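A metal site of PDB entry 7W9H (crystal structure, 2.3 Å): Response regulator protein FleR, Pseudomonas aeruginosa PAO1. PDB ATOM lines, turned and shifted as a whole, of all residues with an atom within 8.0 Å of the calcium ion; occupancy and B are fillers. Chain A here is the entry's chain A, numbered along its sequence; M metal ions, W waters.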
ATOM      1  N   VAL A  12      22.108  15.003  22.121  1.00  0.00           N
ATOM      2  CA  VAL A  12      23.257  15.827  21.767  1.00  0.00           C
ATOM      3  C   VAL A  12      24.368  15.477  22.738  1.00  0.00           C
ATOM      4  O   VAL A  12      24.327  15.863  23.913  1.00  0.00           O
ATOM      5  CB  VAL A  12      22.943  17.327  21.852  1.00  0.00           C
ATOM      6  CG1 VAL A  12      24.147  18.188  21.376  1.00  0.00           C
ATOM      7  CG2 VAL A  12      21.691  17.664  21.078  1.00  0.00           C
ATOM      8  N   GLU A  13      25.384  14.752  22.259  1.00  0.00           N
ATOM      9  CA  GLU A  13      26.434  14.246  23.143  1.00  0.00           C
ATOM     10  C   GLU A  13      27.682  14.007  22.304  1.00  0.00           C
ATOM     11  O   GLU A  13      27.648  13.214  21.364  1.00  0.00           O
ATOM     12  CB  GLU A  13      25.966  12.950  23.840  1.00  0.00           C
ATOM     13  CG  GLU A  13      27.072  12.203  24.603  1.00  0.00           C
ATOM     14  CD  GLU A  13      27.589  12.986  25.819  1.00  0.00           C
ATOM     15  OE1 GLU A  13      26.804  13.165  26.787  1.00  0.00           O
ATOM     16  OE2 GLU A  13      28.761  13.415  25.809  1.00  0.00           O
ATOM     17  N   ASP A  14      28.784  14.677  22.664  1.00  0.00           N
ATOM     18  CA  ASP A  14      30.031  14.527  21.919  1.00  0.00           C
ATOM     19  C   ASP A  14      30.768  13.237  22.241  1.00  0.00           C
ATOM     20  O   ASP A  14      31.617  12.811  21.443  1.00  0.00           O
ATOM     21  CB  ASP A  14      30.952  15.715  22.173  1.00  0.00           C
ATOM     22  CG  ASP A  14      31.220  15.941  23.655  1.00  0.00           C
ATOM     23  OD1 ASP A  14      30.244  16.029  24.426  1.00  0.00           O
ATOM     24  OD2 ASP A  14      32.405  16.033  24.040  1.00  0.00           O
ATOM     25  N   ASP A  15      30.464  12.586  23.361  1.00  0.00           N
ATOM     26  CA  ASP A  15      31.120  11.326  23.722  1.00  0.00           C
ATOM     27  C   ASP A  15      30.436  10.184  22.984  1.00  0.00           C
ATOM     28  O   ASP A  15      29.326   9.776  23.335  1.00  0.00           O
ATOM     29  CB  ASP A  15      31.047  11.092  25.226  1.00  0.00           C
ATOM     30  CG  ASP A  15      31.793   9.828  25.677  1.00  0.00           C
ATOM     31  OD1 ASP A  15      32.647   9.919  26.576  1.00  0.00           O
ATOM     32  OD2 ASP A  15      31.506   8.729  25.150  1.00  0.00           O
ATOM     33  N   LEU A  18      29.067   7.318  25.536  1.00  0.00           N
ATOM     34  CA  LEU A  18      27.806   7.649  26.201  1.00  0.00           C
ATOM     35  C   LEU A  18      26.672   7.861  25.208  1.00  0.00           C
ATOM     36  O   LEU A  18      25.529   7.508  25.496  1.00  0.00           O
ATOM     37  CB  LEU A  18      27.983   8.886  27.087  1.00  0.00           C
ATOM     38  CG  LEU A  18      26.855   9.117  28.100  1.00  0.00           C
ATOM     39  CD1 LEU A  18      27.126   8.369  29.407  1.00  0.00           C
ATOM     40  CD2 LEU A  18      26.711  10.587  28.385  1.00  0.00           C
ATOM     41  N   ASP A  37      26.478  15.052  17.662  1.00  0.00           N
ATOM     42  CA  ASP A  37      27.643  15.173  18.538  1.00  0.00           C
ATOM     43  C   ASP A  37      27.964  16.612  18.913  1.00  0.00           C
ATOM     44  O   ASP A  37      28.937  16.834  19.646  1.00  0.00           O
ATOM     45  CB  ASP A  37      28.862  14.512  17.882  1.00  0.00           C
ATOM     46  CG  ASP A  37      29.147  15.077  16.518  1.00  0.00           C
ATOM     47  OD1 ASP A  37      28.894  14.369  15.514  1.00  0.00           O
ATOM     48  OD2 ASP A  37      29.606  16.239  16.426  1.00  0.00           O
ATOM     49  N   ASP A  57      24.397  17.319  26.405  1.00  0.00           N
ATOM     50  CA  ASP A  57      25.566  17.513  27.232  1.00  0.00           C
ATOM     51  C   ASP A  57      25.842  19.006  27.399  1.00  0.00           C
ATOM     52  O   ASP A  57      25.492  19.831  26.551  1.00  0.00           O
ATOM     53  CB  ASP A  57      26.779  16.818  26.598  1.00  0.00           C
ATOM     54  CG  ASP A  57      28.016  16.849  27.482  1.00  0.00           C
ATOM     55  OD1 ASP A  57      27.876  16.935  28.724  1.00  0.00           O
ATOM     56  OD2 ASP A  57      29.118  16.775  26.925  1.00  0.00           O
ATOM     57  N   VAL A  58      26.471  19.365  28.519  1.00  0.00           N
ATOM     58  CA  VAL A  58      26.831  20.771  28.714  1.00  0.00           C
ATOM     59  C   VAL A  58      28.192  21.084  28.092  1.00  0.00           C
ATOM     60  O   VAL A  58      28.360  22.135  27.460  1.00  0.00           O
ATOM     61  CB  VAL A  58      26.774  21.154  30.212  1.00  0.00           C
ATOM     62  CG1 VAL A  58      27.429  22.500  30.439  1.00  0.00           C
ATOM     63  CG2 VAL A  58      25.331  21.203  30.709  1.00  0.00           C
ATOM     64  N   ASN A  59      29.180  20.203  28.194  1.00  0.00           N
ATOM     65  CA  ASN A  59      30.579  20.532  27.871  1.00  0.00           C
ATOM     66  C   ASN A  59      30.928  19.928  26.520  1.00  0.00           C
ATOM     67  O   ASN A  59      31.216  18.727  26.427  1.00  0.00           O
ATOM     68  CB  ASN A  59      31.516  20.025  28.957  1.00  0.00           C
ATOM     69  CG  ASN A  59      31.114  20.499  30.350  1.00  0.00           C
ATOM     70  OD1 ASN A  59      31.321  21.655  30.717  1.00  0.00           O
ATOM     71  ND2 ASN A  59      30.528  19.590  31.129  1.00  0.00           N
ATOM     72  N   MET A  60      30.914  20.743  25.483  1.00  0.00           N
ATOM     73  CA  MET A  60      31.121  20.181  24.152  1.00  0.00           C
ATOM     74  C   MET A  60      32.142  20.990  23.371  1.00  0.00           C
ATOM     75  O   MET A  60      32.299  22.202  23.589  1.00  0.00           O
ATOM     76  CB  MET A  60      29.802  20.135  23.370  1.00  0.00           C
ATOM     77  CG  MET A  60      28.929  18.996  23.779  1.00  0.00           C
ATOM     78  SD  MET A  60      27.252  19.167  23.148  1.00  0.00           S
ATOM     79  CE  MET A  60      26.963  20.911  23.426  1.00  0.00           C
ATOM     80  N   PRO A  61      32.846  20.344  22.465  1.00  0.00           N
ATOM     81  CA  PRO A  61      33.795  21.065  21.599  1.00  0.00           C
ATOM     82  C   PRO A  61      33.094  21.997  20.627  1.00  0.00           C
ATOM     83  O   PRO A  61      32.855  21.648  19.457  1.00  0.00           O
ATOM     84  CB  PRO A  61      34.522  19.927  20.869  1.00  0.00           C
ATOM     85  CG  PRO A  61      33.527  18.791  20.856  1.00  0.00           C
ATOM     86  CD  PRO A  61      32.799  18.897  22.165  1.00  0.00           C
ATOM     87  N   MET A  84      22.678  17.632  30.781  1.00  0.00           N
ATOM     88  CA  MET A  84      23.484  16.686  31.533  1.00  0.00           C
ATOM     89  C   MET A  84      24.941  17.118  31.519  1.00  0.00           C
ATOM     90  O   MET A  84      25.425  17.722  30.556  1.00  0.00           O
ATOM     91  CB  MET A  84      23.350  15.300  30.957  1.00  0.00           C
ATOM     92  CG  MET A  84      23.424  15.239  29.480  1.00  0.00           C
ATOM     93  SD  MET A  84      23.392  13.505  29.031  1.00  0.00           S
ATOM     94  CE  MET A  84      23.757  13.648  27.275  1.00  0.00           C
ATOM     95  N   THR A  85      25.642  16.808  32.598  1.00  0.00           N
ATOM     96  CA  THR A  85      27.020  17.235  32.687  1.00  0.00           C
ATOM     97  C   THR A  85      27.804  16.301  33.584  1.00  0.00           C
ATOM     98  O   THR A  85      27.262  15.700  34.517  1.00  0.00           O
ATOM     99  CB  THR A  85      27.123  18.686  33.201  1.00  0.00           C
ATOM    100  OG1 THR A  85      28.435  19.195  32.930  1.00  0.00           O
ATOM    101  CG2 THR A  85      26.860  18.774  34.700  1.00  0.00           C
ATOM    102  N   ALA A  86      29.096  16.180  33.278  1.00  0.00           N
ATOM    103  CA  ALA A  86      30.006  15.473  34.168  1.00  0.00           C
ATOM    104  C   ALA A  86      30.432  16.359  35.338  1.00  0.00           C
ATOM    105  O   ALA A  86      30.645  15.873  36.443  1.00  0.00           O
ATOM    106  CB  ALA A  86      31.221  14.989  33.378  1.00  0.00           C
ATOM    107  N   TYR A  87      30.503  17.665  35.107  1.00  0.00           N
ATOM    108  CA  TYR A  87      30.957  18.631  36.095  1.00  0.00           C
ATOM    109  C   TYR A  87      29.752  19.461  36.518  1.00  0.00           C
ATOM    110  O   TYR A  87      29.429  20.495  35.926  1.00  0.00           O
ATOM    111  CB  TYR A  87      32.074  19.503  35.492  1.00  0.00           C
ATOM    112  CG  TYR A  87      32.923  18.803  34.447  1.00  0.00           C
ATOM    113  CD1 TYR A  87      33.139  19.391  33.192  1.00  0.00           C
ATOM    114  CD2 TYR A  87      33.515  17.555  34.687  1.00  0.00           C
ATOM    115  CE1 TYR A  87      33.926  18.762  32.222  1.00  0.00           C
ATOM    116  CE2 TYR A  87      34.293  16.917  33.724  1.00  0.00           C
ATOM    117  CZ  TYR A  87      34.489  17.528  32.490  1.00  0.00           C
ATOM    118  OH  TYR A  87      35.260  16.913  31.533  1.00  0.00           O
ATOM    119  N   LYS A 107      26.241  13.388  35.490  1.00  0.00           N
ATOM    120  CA  LYS A 107      26.535  12.044  35.013  1.00  0.00           C
ATOM    121  C   LYS A 107      27.309  11.254  36.068  1.00  0.00           C
ATOM    122  O   LYS A 107      28.108  11.823  36.806  1.00  0.00           O
ATOM    123  CB  LYS A 107      27.345  12.080  33.719  1.00  0.00           C
ATOM    124  CG  LYS A 107      26.682  12.740  32.541  1.00  0.00           C
ATOM    125  CD  LYS A 107      27.762  13.101  31.539  1.00  0.00           C
ATOM    126  CE  LYS A 107      27.167  13.614  30.231  1.00  0.00           C
ATOM    127  NZ  LYS A 107      28.244  13.874  29.257  1.00  0.00           N
HETATM  128 CA    CA M   1      31.298  16.432  26.309  1.00  0.00          CA
HETATM  129  O   HOH W   1      31.231  16.264  28.740  1.00  0.00           O
HETATM  130  O   HOH W   2      30.928  14.295  26.808  1.00  0.00           O
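The side-chain amino group (NZ) of Lys 107 lies within salt-bridge range of the side-chain carboxylate (OE1) of Glu 13. N of Asp 57 lies within hydrogen-bond range of O of Val 12 (2.9 Å). The side-chain hydroxyl (OG1) of Thr 85 sits at hydrogen-bond distance from the side-chain amide nitrogen (ND2) of Asn 59 (2.8 Å). The backbone NH (N) of Asp 15 is in hydrogen-bond range of the side-chain carboxylate (OE2) of Glu 13. The side-chain carboxylate (OD1) of Asp 57 is in salt-bridge range of the side-chain amino group (NZ) of Lys 107, 3.1 Å away.
Residues that only touch the calcium ion: Glu 13 (3.97 Å). The nearest printed residue that does not touch the calcium ion is Met 60 (4.3 Å).
The calcium ion is bound by OD1 of Asp 14, water W2, OD2 of Asp 57, O of Asn 59, water W1 and OD2 of Asp 14. The calcium ion has six donor atoms within binding distance.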
